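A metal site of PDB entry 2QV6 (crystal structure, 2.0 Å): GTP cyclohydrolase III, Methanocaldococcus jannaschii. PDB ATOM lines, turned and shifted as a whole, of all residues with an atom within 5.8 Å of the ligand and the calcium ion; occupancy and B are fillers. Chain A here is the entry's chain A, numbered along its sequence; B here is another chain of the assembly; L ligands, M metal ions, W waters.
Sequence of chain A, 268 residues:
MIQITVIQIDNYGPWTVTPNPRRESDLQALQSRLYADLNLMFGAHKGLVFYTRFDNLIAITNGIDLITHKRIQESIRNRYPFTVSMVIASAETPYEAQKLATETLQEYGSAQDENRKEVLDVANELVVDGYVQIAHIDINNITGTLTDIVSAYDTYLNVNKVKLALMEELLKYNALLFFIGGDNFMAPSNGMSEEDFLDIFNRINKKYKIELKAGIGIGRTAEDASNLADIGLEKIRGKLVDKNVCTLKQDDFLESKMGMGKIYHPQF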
ATOM      1  N   HIS A 136       5.558  28.224  12.053  1.00  0.00           N
ATOM      2  CA  HIS A 136       5.845  27.963  13.455  1.00  0.00           C
ATOM      3  C   HIS A 136       6.696  26.694  13.470  1.00  0.00           C
ATOM      4  O   HIS A 136       6.205  25.594  13.241  1.00  0.00           O
ATOM      5  CB  HIS A 136       4.500  27.783  14.203  1.00  0.00           C
ATOM      6  CG  HIS A 136       4.624  27.669  15.682  1.00  0.00           C
ATOM      7  ND1 HIS A 136       3.521  27.651  16.518  1.00  0.00           N
ATOM      8  CD2 HIS A 136       5.710  27.571  16.485  1.00  0.00           C
ATOM      9  CE1 HIS A 136       3.928  27.529  17.761  1.00  0.00           C
ATOM     10  NE2 HIS A 136       5.254  27.500  17.780  1.00  0.00           N
ATOM     11  N   ASP A 138       9.473  23.973  15.149  1.00  0.00           N
ATOM     12  CA  ASP A 138       9.564  23.290  16.424  1.00  0.00           C
ATOM     13  C   ASP A 138      10.507  22.068  16.251  1.00  0.00           C
ATOM     14  O   ASP A 138      10.600  21.516  15.178  1.00  0.00           O
ATOM     15  CB  ASP A 138       8.127  22.883  16.876  1.00  0.00           C
ATOM     16  CG  ASP A 138       8.100  21.902  18.052  1.00  0.00           C
ATOM     17  OD1 ASP A 138       8.382  22.307  19.200  1.00  0.00           O
ATOM     18  OD2 ASP A 138       7.775  20.719  17.860  1.00  0.00           O
ATOM     19  N   ILE A 139      11.188  21.667  17.303  1.00  0.00           N
ATOM     20  CA  ILE A 139      12.049  20.493  17.276  1.00  0.00           C
ATOM     21  C   ILE A 139      11.250  19.225  17.664  1.00  0.00           C
ATOM     22  O   ILE A 139      10.354  19.278  18.525  1.00  0.00           O
ATOM     23  CB  ILE A 139      13.277  20.726  18.218  1.00  0.00           C
ATOM     24  CG1 ILE A 139      14.171  21.823  17.618  1.00  0.00           C
ATOM     25  CG2 ILE A 139      14.056  19.447  18.418  1.00  0.00           C
ATOM     26  CD1 ILE A 139      15.178  22.418  18.562  1.00  0.00           C
ATOM     27  N   ASN A 140      11.509  18.111  16.986  1.00  0.00           N
ATOM     28  CA  ASN A 140      10.807  16.847  17.270  1.00  0.00           C
ATOM     29  C   ASN A 140      11.439  16.231  18.486  1.00  0.00           C
ATOM     30  O   ASN A 140      12.640  16.061  18.529  1.00  0.00           O
ATOM     31  CB  ASN A 140      10.884  15.869  16.081  1.00  0.00           C
ATOM     32  CG  ASN A 140       9.949  16.234  14.946  1.00  0.00           C
ATOM     33  OD1 ASN A 140       9.072  17.084  15.097  1.00  0.00           O
ATOM     34  ND2 ASN A 140      10.116  15.591  13.809  1.00  0.00           N
ATOM     35  N   ASN A 141      10.630  15.932  19.479  1.00  0.00           N
ATOM     36  CA  ASN A 141      11.081  15.281  20.699  1.00  0.00           C
ATOM     37  C   ASN A 141      12.260  15.956  21.383  1.00  0.00           C
ATOM     38  O   ASN A 141      13.250  15.291  21.726  1.00  0.00           O
ATOM     39  CB  ASN A 141      11.395  13.803  20.445  1.00  0.00           C
ATOM     40  CG  ASN A 141      11.579  13.010  21.738  1.00  0.00           C
ATOM     41  OD1 ASN A 141      11.072  13.392  22.803  1.00  0.00           O
ATOM     42  ND2 ASN A 141      12.330  11.903  21.654  1.00  0.00           N
ATOM     43  N   ILE A 142      12.138  17.250  21.666  1.00  0.00           N
ATOM     44  CA  ILE A 142      13.148  17.945  22.498  1.00  0.00           C
ATOM     45  C   ILE A 142      13.266  17.332  23.909  1.00  0.00           C
ATOM     46  O   ILE A 142      14.356  17.315  24.482  1.00  0.00           O
ATOM     47  CB  ILE A 142      12.896  19.484  22.625  1.00  0.00           C
ATOM     48  CG1 ILE A 142      14.130  20.208  23.209  1.00  0.00           C
ATOM     49  CG2 ILE A 142      11.681  19.800  23.504  1.00  0.00           C
ATOM     50  CD1 ILE A 142      15.146  20.591  22.208  1.00  0.00           C
ATOM     51  N   THR A 143      12.179  16.818  24.464  1.00  0.00           N
ATOM     52  CA  THR A 143      12.181  16.410  25.886  1.00  0.00           C
ATOM     53  C   THR A 143      12.966  15.118  26.066  1.00  0.00           C
ATOM     54  O   THR A 143      13.790  14.985  27.004  1.00  0.00           O
ATOM     55  CB  THR A 143      10.747  16.267  26.444  1.00  0.00           C
ATOM     56  OG1 THR A 143       9.982  17.415  26.112  1.00  0.00           O
ATOM     57  CG2 THR A 143      10.768  16.115  27.972  1.00  0.00           C
ATOM     58  N   GLY A 144      12.740  14.171  25.158  1.00  0.00           N
ATOM     59  CA  GLY A 144      13.402  12.861  25.219  1.00  0.00           C
ATOM     60  C   GLY A 144      14.828  12.860  24.715  1.00  0.00           C
ATOM     61  O   GLY A 144      15.632  12.046  25.159  1.00  0.00           O
ATOM     62  N   ILE A 180      10.659  31.985  20.394  1.00  0.00           N
ATOM     63  CA  ILE A 180       9.464  32.253  21.209  1.00  0.00           C
ATOM     64  C   ILE A 180       9.362  31.400  22.496  1.00  0.00           C
ATOM     65  O   ILE A 180       8.387  31.493  23.248  1.00  0.00           O
ATOM     66  CB  ILE A 180       8.161  32.288  20.327  1.00  0.00           C
ATOM     67  CG1 ILE A 180       7.998  31.034  19.480  1.00  0.00           C
ATOM     68  CG2 ILE A 180       8.240  33.497  19.400  1.00  0.00           C
ATOM     69  CD1 ILE A 180       6.573  30.472  19.421  1.00  0.00           C
ATOM     70  N   GLY A 181      10.430  30.685  22.809  1.00  0.00           N
ATOM     71  CA  GLY A 181      10.528  29.905  24.028  1.00  0.00           C
ATOM     72  C   GLY A 181      10.524  28.432  23.697  1.00  0.00           C
ATOM     73  O   GLY A 181       9.981  27.996  22.648  1.00  0.00           O
ATOM     74  N   GLY A 182      11.115  27.664  24.589  1.00  0.00           N
ATOM     75  CA  GLY A 182      11.149  26.231  24.479  1.00  0.00           C
ATOM     76  C   GLY A 182      12.115  25.756  23.419  1.00  0.00           C
ATOM     77  O   GLY A 182      13.311  25.976  23.496  1.00  0.00           O
ATOM     78  N   ASP A 183      11.559  25.067  22.423  1.00  0.00           N
ATOM     79  CA  ASP A 183      12.284  24.697  21.234  1.00  0.00           C
ATOM     80  C   ASP A 183      11.515  25.299  20.047  1.00  0.00           C
ATOM     81  O   ASP A 183      11.476  24.705  18.992  1.00  0.00           O
ATOM     82  CB  ASP A 183      12.375  23.172  21.135  1.00  0.00           C
ATOM     83  CG  ASP A 183      11.024  22.472  21.212  1.00  0.00           C
ATOM     84  OD1 ASP A 183      10.102  22.971  21.899  1.00  0.00           O
ATOM     85  OD2 ASP A 183      10.849  21.397  20.595  1.00  0.00           O
ATOM     86  N   ASN A 184      10.918  26.472  20.253  1.00  0.00           N
ATOM     87  CA  ASN A 184       9.976  27.066  19.310  1.00  0.00           C
ATOM     88  C   ASN A 184      10.511  28.338  18.681  1.00  0.00           C
ATOM     89  O   ASN A 184      11.159  29.133  19.342  1.00  0.00           O
ATOM     90  CB  ASN A 184       8.647  27.360  19.999  1.00  0.00           C
ATOM     91  CG  ASN A 184       7.796  26.135  20.224  1.00  0.00           C
ATOM     92  OD1 ASN A 184       8.106  25.292  21.066  1.00  0.00           O
ATOM     93  ND2 ASN A 184       6.667  26.048  19.513  1.00  0.00           N
ATOM     94  N   LYS A 213       9.955  20.444  12.433  1.00  0.00           N
ATOM     95  CA  LYS A 213       8.670  20.431  11.738  1.00  0.00           C
ATOM     96  C   LYS A 213       8.081  21.840  11.765  1.00  0.00           C
ATOM     97  O   LYS A 213       8.527  22.691  12.519  1.00  0.00           O
ATOM     98  CB  LYS A 213       7.719  19.398  12.370  1.00  0.00           C
ATOM     99  CG  LYS A 213       7.548  19.567  13.880  1.00  0.00           C
ATOM    100  CD  LYS A 213       6.432  18.670  14.452  1.00  0.00           C
ATOM    101  CE  LYS A 213       6.198  18.918  15.953  1.00  0.00           C
ATOM    102  NZ  LYS A 213       7.357  18.504  16.845  1.00  0.00           N
ATOM    103  N   ASP A 230      -0.476  27.041  14.292  1.00  0.00           N
ATOM    104  CA  ASP A 230      -0.568  26.148  15.463  1.00  0.00           C
ATOM    105  C   ASP A 230      -1.362  24.870  15.159  1.00  0.00           C
ATOM    106  O   ASP A 230      -1.008  23.777  15.605  1.00  0.00           O
ATOM    107  CB  ASP A 230      -1.235  26.855  16.652  1.00  0.00           C
ATOM    108  CG  ASP A 230      -0.312  27.810  17.390  1.00  0.00           C
ATOM    109  OD1 ASP A 230       0.927  27.641  17.394  1.00  0.00           O
ATOM    110  OD2 ASP A 230      -0.829  28.757  18.015  1.00  0.00           O
ATOM    111  N   ARG A 237       1.537  16.419  14.478  1.00  0.00           N
ATOM    112  CA  ARG A 237       1.606  15.572  15.662  1.00  0.00           C
ATOM    113  C   ARG A 237       0.626  14.399  15.640  1.00  0.00           C
ATOM    114  O   ARG A 237       0.971  13.302  16.066  1.00  0.00           O
ATOM    115  CB  ARG A 237       1.364  16.379  16.932  1.00  0.00           C
ATOM    116  CG  ARG A 237       2.506  17.259  17.298  1.00  0.00           C
ATOM    117  CD  ARG A 237       2.470  17.616  18.753  1.00  0.00           C
ATOM    118  NE  ARG A 237       3.666  18.401  19.081  1.00  0.00           N
ATOM    119  CZ  ARG A 237       3.686  19.710  19.282  1.00  0.00           C
ATOM    120  NH1 ARG A 237       2.581  20.443  19.211  1.00  0.00           N
ATOM    121  NH2 ARG A 237       4.837  20.299  19.563  1.00  0.00           N
ATOM    122  N   TYR B  12       4.732  21.758  30.899  1.00  0.00           N
ATOM    123  CA  TYR B  12       4.370  23.005  30.252  1.00  0.00           C
ATOM    124  C   TYR B  12       3.886  22.712  28.839  1.00  0.00           C
ATOM    125  O   TYR B  12       2.842  23.186  28.457  1.00  0.00           O
ATOM    126  CB  TYR B  12       5.543  23.999  30.290  1.00  0.00           C
ATOM    127  CG  TYR B  12       5.208  25.380  29.785  1.00  0.00           C
ATOM    128  CD1 TYR B  12       4.074  26.072  30.247  1.00  0.00           C
ATOM    129  CD2 TYR B  12       5.993  25.996  28.807  1.00  0.00           C
ATOM    130  CE1 TYR B  12       3.751  27.352  29.755  1.00  0.00           C
ATOM    131  CE2 TYR B  12       5.664  27.264  28.316  1.00  0.00           C
ATOM    132  CZ  TYR B  12       4.557  27.943  28.794  1.00  0.00           C
ATOM    133  OH  TYR B  12       4.243  29.192  28.275  1.00  0.00           O
ATOM    134  N   GLY B  13       4.614  21.902  28.103  1.00  0.00           N
ATOM    135  CA  GLY B  13       4.254  21.571  26.706  1.00  0.00           C
ATOM    136  C   GLY B  13       2.819  21.099  26.441  1.00  0.00           C
ATOM    137  O   GLY B  13       2.170  21.607  25.519  1.00  0.00           O
ATOM    138  N   PRO B  14       2.339  20.090  27.201  1.00  0.00           N
ATOM    139  CA  PRO B  14       0.924  19.698  27.131  1.00  0.00           C
ATOM    140  C   PRO B  14      -0.109  20.762  27.523  1.00  0.00           C
ATOM    141  O   PRO B  14      -1.202  20.773  26.964  1.00  0.00           O
ATOM    142  CB  PRO B  14       0.845  18.514  28.077  1.00  0.00           C
ATOM    143  CG  PRO B  14       2.235  17.958  28.109  1.00  0.00           C
ATOM    144  CD  PRO B  14       3.109  19.169  28.039  1.00  0.00           C
ATOM    145  N   THR B  16       0.048  24.012  26.928  1.00  0.00           N
ATOM    146  CA  THR B  16      -0.046  25.019  25.855  1.00  0.00           C
ATOM    147  C   THR B  16      -0.947  24.598  24.710  1.00  0.00           C
ATOM    148  O   THR B  16      -1.301  25.432  23.871  1.00  0.00           O
ATOM    149  CB  THR B  16       1.354  25.374  25.241  1.00  0.00           C
ATOM    150  OG1 THR B  16       1.889  24.243  24.540  1.00  0.00           O
ATOM    151  CG2 THR B  16       2.378  25.786  26.298  1.00  0.00           C
ATOM    152  N   VAL B  17      -1.301  23.306  24.646  1.00  0.00           N
ATOM    153  CA  VAL B  17      -2.149  22.746  23.576  1.00  0.00           C
ATOM    154  C   VAL B  17      -3.387  21.968  24.064  1.00  0.00           C
ATOM    155  O   VAL B  17      -4.185  21.469  23.250  1.00  0.00           O
ATOM    156  CB  VAL B  17      -1.319  21.817  22.637  1.00  0.00           C
ATOM    157  CG1 VAL B  17      -0.279  22.628  21.834  1.00  0.00           C
ATOM    158  CG2 VAL B  17      -0.642  20.717  23.442  1.00  0.00           C
ATOM    159  N   ARG B  22      -3.083  27.919  22.111  1.00  0.00           N
ATOM    160  CA  ARG B  22      -3.393  29.226  22.690  1.00  0.00           C
ATOM    161  C   ARG B  22      -2.766  30.346  21.882  1.00  0.00           C
ATOM    162  O   ARG B  22      -1.648  30.199  21.441  1.00  0.00           O
ATOM    163  CB  ARG B  22      -2.830  29.260  24.079  1.00  0.00           C
ATOM    164  CG  ARG B  22      -3.339  28.141  24.966  1.00  0.00           C
ATOM    165  CD  ARG B  22      -2.758  28.196  26.336  1.00  0.00           C
ATOM    166  NE  ARG B  22      -3.088  26.989  27.088  1.00  0.00           N
ATOM    167  CZ  ARG B  22      -4.189  26.803  27.828  1.00  0.00           C
ATOM    168  NH1 ARG B  22      -5.095  27.747  27.975  1.00  0.00           N
ATOM    169  NH2 ARG B  22      -4.364  25.648  28.462  1.00  0.00           N
ATOM    170  N   GLU B  24      -0.582  33.083  20.565  1.00  0.00           N
ATOM    171  CA  GLU B  24       0.831  33.259  20.878  1.00  0.00           C
ATOM    172  C   GLU B  24       1.160  34.562  21.623  1.00  0.00           C
ATOM    173  O   GLU B  24       1.998  34.545  22.521  1.00  0.00           O
ATOM    174  CB  GLU B  24       1.683  33.152  19.609  1.00  0.00           C
ATOM    175  CG  GLU B  24       3.190  33.049  19.844  1.00  0.00           C
ATOM    176  CD  GLU B  24       3.590  31.887  20.762  1.00  0.00           C
ATOM    177  OE1 GLU B  24       3.053  30.756  20.645  1.00  0.00           O
ATOM    178  OE2 GLU B  24       4.469  32.101  21.619  1.00  0.00           O
ATOM    179  N   LEU B  27       0.822  33.907  25.172  1.00  0.00           N
ATOM    180  CA  LEU B  27       1.906  33.065  25.677  1.00  0.00           C
ATOM    181  C   LEU B  27       3.171  33.875  25.889  1.00  0.00           C
ATOM    182  O   LEU B  27       3.913  33.634  26.843  1.00  0.00           O
ATOM    183  CB  LEU B  27       2.180  31.865  24.753  1.00  0.00           C
ATOM    184  CG  LEU B  27       1.148  30.715  24.762  1.00  0.00           C
ATOM    185  CD1 LEU B  27       1.646  29.582  23.912  1.00  0.00           C
ATOM    186  CD2 LEU B  27       0.816  30.190  26.160  1.00  0.00           C
ATOM    187  N   GLN B  28       3.390  34.875  25.033  1.00  0.00           N
ATOM    188  CA  GLN B  28       4.521  35.781  25.190  1.00  0.00           C
ATOM    189  C   GLN B  28       4.406  36.685  26.410  1.00  0.00           C
ATOM    190  O   GLN B  28       5.387  36.837  27.166  1.00  0.00           O
ATOM    191  CB  GLN B  28       4.753  36.609  23.917  1.00  0.00           C
ATOM    192  CG  GLN B  28       5.141  35.753  22.757  1.00  0.00           C
ATOM    193  CD  GLN B  28       6.401  34.948  23.000  1.00  0.00           C
ATOM    194  OE1 GLN B  28       6.396  33.714  22.921  1.00  0.00           O
ATOM    195  NE2 GLN B  28       7.489  35.631  23.263  1.00  0.00           N
ATOM    196  N   GLN B  31       4.818  34.369  29.566  1.00  0.00           N
ATOM    197  CA  GLN B  31       6.224  33.959  29.789  1.00  0.00           C
ATOM    198  C   GLN B  31       7.126  35.072  30.310  1.00  0.00           C
ATOM    199  O   GLN B  31       7.972  34.845  31.219  1.00  0.00           O
ATOM    200  CB  GLN B  31       6.803  33.313  28.515  1.00  0.00           C
ATOM    201  CG  GLN B  31       6.424  31.836  28.381  1.00  0.00           C
ATOM    202  CD  GLN B  31       6.647  31.236  26.993  1.00  0.00           C
ATOM    203  OE1 GLN B  31       7.321  31.819  26.158  1.00  0.00           O
ATOM    204  NE2 GLN B  31       6.136  30.060  26.782  1.00  0.00           N
ATOM    205  N   ARG B  53      15.586  29.677  28.258  1.00  0.00           N
ATOM    206  CA  ARG B  53      14.571  29.218  27.269  1.00  0.00           C
ATOM    207  C   ARG B  53      13.110  29.533  27.621  1.00  0.00           C
ATOM    208  O   ARG B  53      12.181  29.103  26.903  1.00  0.00           O
ATOM    209  CB  ARG B  53      14.719  27.721  27.014  1.00  0.00           C
ATOM    210  CG  ARG B  53      16.141  27.343  26.635  1.00  0.00           C
ATOM    211  CD  ARG B  53      16.207  26.036  25.889  1.00  0.00           C
ATOM    212  NE  ARG B  53      15.949  24.899  26.772  1.00  0.00           N
ATOM    213  CZ  ARG B  53      14.926  24.050  26.631  1.00  0.00           C
ATOM    214  NH1 ARG B  53      14.078  24.140  25.599  1.00  0.00           N
ATOM    215  NH2 ARG B  53      14.786  23.065  27.486  1.00  0.00           N
ATOM    216  N   ASP B  55      10.669  28.441  29.321  1.00  0.00           N
ATOM    217  CA  ASP B  55      10.180  27.277  30.083  1.00  0.00           C
ATOM    218  C   ASP B  55      11.234  26.658  31.031  1.00  0.00           C
ATOM    219  O   ASP B  55      10.866  25.863  31.882  1.00  0.00           O
ATOM    220  CB  ASP B  55       9.621  26.176  29.191  1.00  0.00           C
ATOM    221  CG  ASP B  55      10.699  25.405  28.409  1.00  0.00           C
ATOM    222  OD1 ASP B  55      11.733  25.996  28.050  1.00  0.00           O
ATOM    223  OD2 ASP B  55      10.524  24.187  28.154  1.00  0.00           O
ATOM    224  N   ASN B  56      12.519  26.999  30.841  1.00  0.00           N
ATOM    225  CA  ASN B  56      13.639  26.623  31.757  1.00  0.00           C
ATOM    226  C   ASN B  56      14.500  27.856  32.039  1.00  0.00           C
ATOM    227  O   ASN B  56      14.926  28.493  31.092  1.00  0.00           O
ATOM    228  CB  ASN B  56      14.557  25.562  31.109  1.00  0.00           C
ATOM    229  CG  ASN B  56      13.975  24.153  31.097  1.00  0.00           C
ATOM    230  OD1 ASN B  56      14.255  23.362  31.987  1.00  0.00           O
ATOM    231  ND2 ASN B  56      13.187  23.831  30.087  1.00  0.00           N
ATOM    232  N   GLN B 112       7.833  16.461  31.188  1.00  0.00           N
ATOM    233  CA  GLN B 112       6.427  16.303  30.775  1.00  0.00           C
ATOM    234  C   GLN B 112       5.782  15.092  31.446  1.00  0.00           C
ATOM    235  O   GLN B 112       5.176  14.254  30.806  1.00  0.00           O
ATOM    236  CB  GLN B 112       6.354  16.228  29.248  1.00  0.00           C
ATOM    237  CG  GLN B 112       6.864  17.492  28.572  1.00  0.00           C
ATOM    238  CD  GLN B 112       6.547  17.547  27.099  1.00  0.00           C
ATOM    239  OE1 GLN B 112       6.019  16.604  26.539  1.00  0.00           O
ATOM    240  NE2 GLN B 112       6.885  18.665  26.467  1.00  0.00           N
HETATM  241  P1  LIG L   1       6.956  17.107  20.226  1.00  0.00           P
HETATM  242  O1  LIG L   1       5.500  16.749  20.131  1.00  0.00           O
HETATM  243  O2  LIG L   1       7.828  16.215  19.406  1.00  0.00           O
HETATM  244  O3  LIG L   1       7.348  18.481  19.825  1.00  0.00           O
HETATM  245  O4  LIG L   1       7.360  16.888  21.795  1.00  0.00           O
HETATM  246  P2  LIG L   1       8.438  17.808  22.502  1.00  0.00           P
HETATM  247  O5  LIG L   1       9.343  18.575  21.582  1.00  0.00           O
HETATM  248  O6  LIG L   1       9.228  17.111  23.636  1.00  0.00           O
HETATM  249  O7  LIG L   1       7.708  18.865  23.492  1.00  0.00           O
HETATM  250  P3  LIG L   1       6.937  20.215  23.144  1.00  0.00           P
HETATM  251  O8  LIG L   1       5.443  19.920  23.093  1.00  0.00           O
HETATM  252  O9  LIG L   1       7.398  20.859  21.862  1.00  0.00           O
HETATM  253  O10 LIG L   1       7.209  21.175  24.372  1.00  0.00           O
HETATM  254  C1  LIG L   1       8.492  21.613  24.709  1.00  0.00           C
HETATM  255  C2  LIG L   1       8.382  23.121  24.954  1.00  0.00           C
HETATM  256  O11 LIG L   1       7.805  23.788  23.826  1.00  0.00           O
HETATM  257  C3  LIG L   1       7.502  23.520  26.108  1.00  0.00           C
HETATM  258  O12 LIG L   1       8.192  23.427  27.350  1.00  0.00           O
HETATM  259  C4  LIG L   1       7.178  24.941  25.755  1.00  0.00           C
HETATM  260  O13 LIG L   1       8.212  25.746  26.263  1.00  0.00           O
HETATM  261  C5  LIG L   1       7.260  25.027  24.250  1.00  0.00           C
HETATM  262  N1  LIG L   1       6.000  25.276  23.509  1.00  0.00           N
HETATM  263  C6  LIG L   1       5.071  24.345  23.093  1.00  0.00           C
HETATM  264  N2  LIG L   1       4.116  24.981  22.369  1.00  0.00           N
HETATM  265  C7  LIG L   1       4.436  26.288  22.324  1.00  0.00           C
HETATM  266  C8  LIG L   1       3.800  27.346  21.728  1.00  0.00           C
HETATM  267  O14 LIG L   1       2.713  27.259  21.088  1.00  0.00           O
HETATM  268  N3  LIG L   1       4.383  28.579  21.829  1.00  0.00           N
HETATM  269  C9  LIG L   1       5.536  28.803  22.510  1.00  0.00           C
HETATM  270  N4  LIG L   1       5.925  30.078  22.496  1.00  0.00           N
HETATM  271  N5  LIG L   1       6.216  27.765  23.131  1.00  0.00           N
HETATM  272  C10 LIG L   1       5.641  26.501  23.003  1.00  0.00           C
HETATM  273 CA    CA M   1       8.852  20.107  19.990  1.00  0.00          CA
HETATM  274  O   HOH W   1       3.230  21.209  22.843  1.00  0.00           O
HETATM  275  O   HOH W   2       7.730  28.323  25.508  1.00  0.00           O
HETATM  276  O   HOH W   3       7.340  20.807  28.484  1.00  0.00           O
HETATM  277  O   HOH W   4      -0.324  26.724  21.657  1.00  0.00           O
HETATM  278  O   HOH W   5      10.532  22.001  29.469  1.00  0.00           O
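An oxygen (O6) of the ligand lies within hydrogen-bond range of the side-chain hydroxyl of Thr 143, 2.6 Å away.
The side-chain hydroxyl of Thr 16 of chain B lies within hydrogen-bond range of a nitrogen (N2) of the ligand.
N of Asn 141 lies within hydrogen-bond range of O2 of the ligand, at 2.8 Å.
O2 of the ligand lies within salt-bridge range of NZ of Lys 213.
N4 of the ligand sits at hydrogen-bond distance from O of Ile 180.
OD2 of Asp 55 of chain B is in hydrogen-bond range of O12 of the ligand (2.6 Å).
OE2 of Glu 24 of chain B lies within hydrogen-bond range of N4 of the ligand.
The side-chain amide oxygen of Asn 184 sits close to an oxygen (O11) of the ligand (3.2 Å).
An oxygen (O6) of the ligand sits at hydrogen-bond distance from the backbone NH (N) of Thr 143 (3.1 Å).
An oxygen (O7) of the ligand lies within hydrogen-bond range of the side-chain amide nitrogen (NE2) of Gln 112 of chain B, 3.1 Å away.
The backbone NH (N) of Ile 142 sits close to an oxygen (O5) of the ligand, at 3.1 Å.
An oxygen (O1) of the ligand is in salt-bridge range of the guanidinium group (NE) of Arg 237, at 2.7 Å.
The side-chain amide oxygen (OE1) of Gln 31 of chain B sits close to the backbone carbonyl oxygen (O) of Ile 180 (3.1 Å).
The backbone carbonyl oxygen (O) of Ile 180 lies close to the side-chain amide oxygen (OE1) of Gln 28 of chain B (3.0 Å).
The guanidinium group of Arg 53 of chain B lies within salt-bridge range of the side-chain carboxylate of Asp 55 of chain B, at 3.9 Å.
The side-chain hydroxyl (OG1) of Thr 16 of chain B is in hydrogen-bond range of the backbone carbonyl oxygen (O) of Gly 13 of chain B (2.8 Å).
The side-chain carboxylate (OD1) of Asp 183 sits close to the side-chain amide oxygen (OD1) of Asn 184, 3.2 Å away.
The backbone carbonyl oxygen (O) of Gly 182 lies within hydrogen-bond range of the guanidinium group (NH1) of Arg 53 of chain B (2.9 Å).
A ring nitrogen (ND1) of His 136 sits at hydrogen-bond distance from the side-chain carboxylate (OD1) of Asp 230.
The side-chain amide nitrogen of Asn 56 of chain B is in hydrogen-bond range of the side-chain carboxylate of Asp 55 of chain B.
Residues that only touch the ligand: His 136 (3.6 Å), Asn 140 (3.7 Å), Gly 181 (3.8 Å), Gly 182 (3.5 Å), Tyr 12 of chain B (3.4 Å), Gly 13 of chain B (3.8 Å), Leu 27 of chain B (3.6 Å) and Gln 28 of chain B (3.7 Å).
Hydrophobic or aromatic side chains that line the ligand: His 136, Ile 142, Ile 180, Tyr 12 of chain B and Leu 27 of chain B.
Of the 30 residues printed, 22 come within 4 Å of the ligand.
Residues that only touch the calcium ion: Lys 213.
Of the 30 residues printed, 4 come within 4 Å of the calcium ion.
The calcium ion is bound by O3 of the ligand, O of Ile 139, O5 of the ligand, OD1 of Asp 138, OD2 of Asp 183, OD2 of Asp 138 and O9 of the ligand.
Water W1 lies within hydrogen-bond range of O8 of the ligand (2.6 Å) and O of Gly 13 of chain B (2.9 Å).
Water W2 bridges the side-chain amide nitrogen (NE2) of Gln 31 of chain B and an oxygen (O13) of the ligand.
Water W3 lies within hydrogen-bond range of N of Gly 13 of chain B, NE2 of Gln 112 of chain B and O12 of the ligand.
Water W4 lies within hydrogen-bond range of O of Thr 16 of chain B, N of Arg 22 of chain B and O14 of the ligand.
Water W5 lies within hydrogen-bond range of the side-chain carboxylate (OD2) of Asp 55 of chain B (2.6 Å), the side-chain amide nitrogen (ND2) of Asn 56 of chain B (3.3 Å) and an oxygen (O12) of the ligand (3.5 Å).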
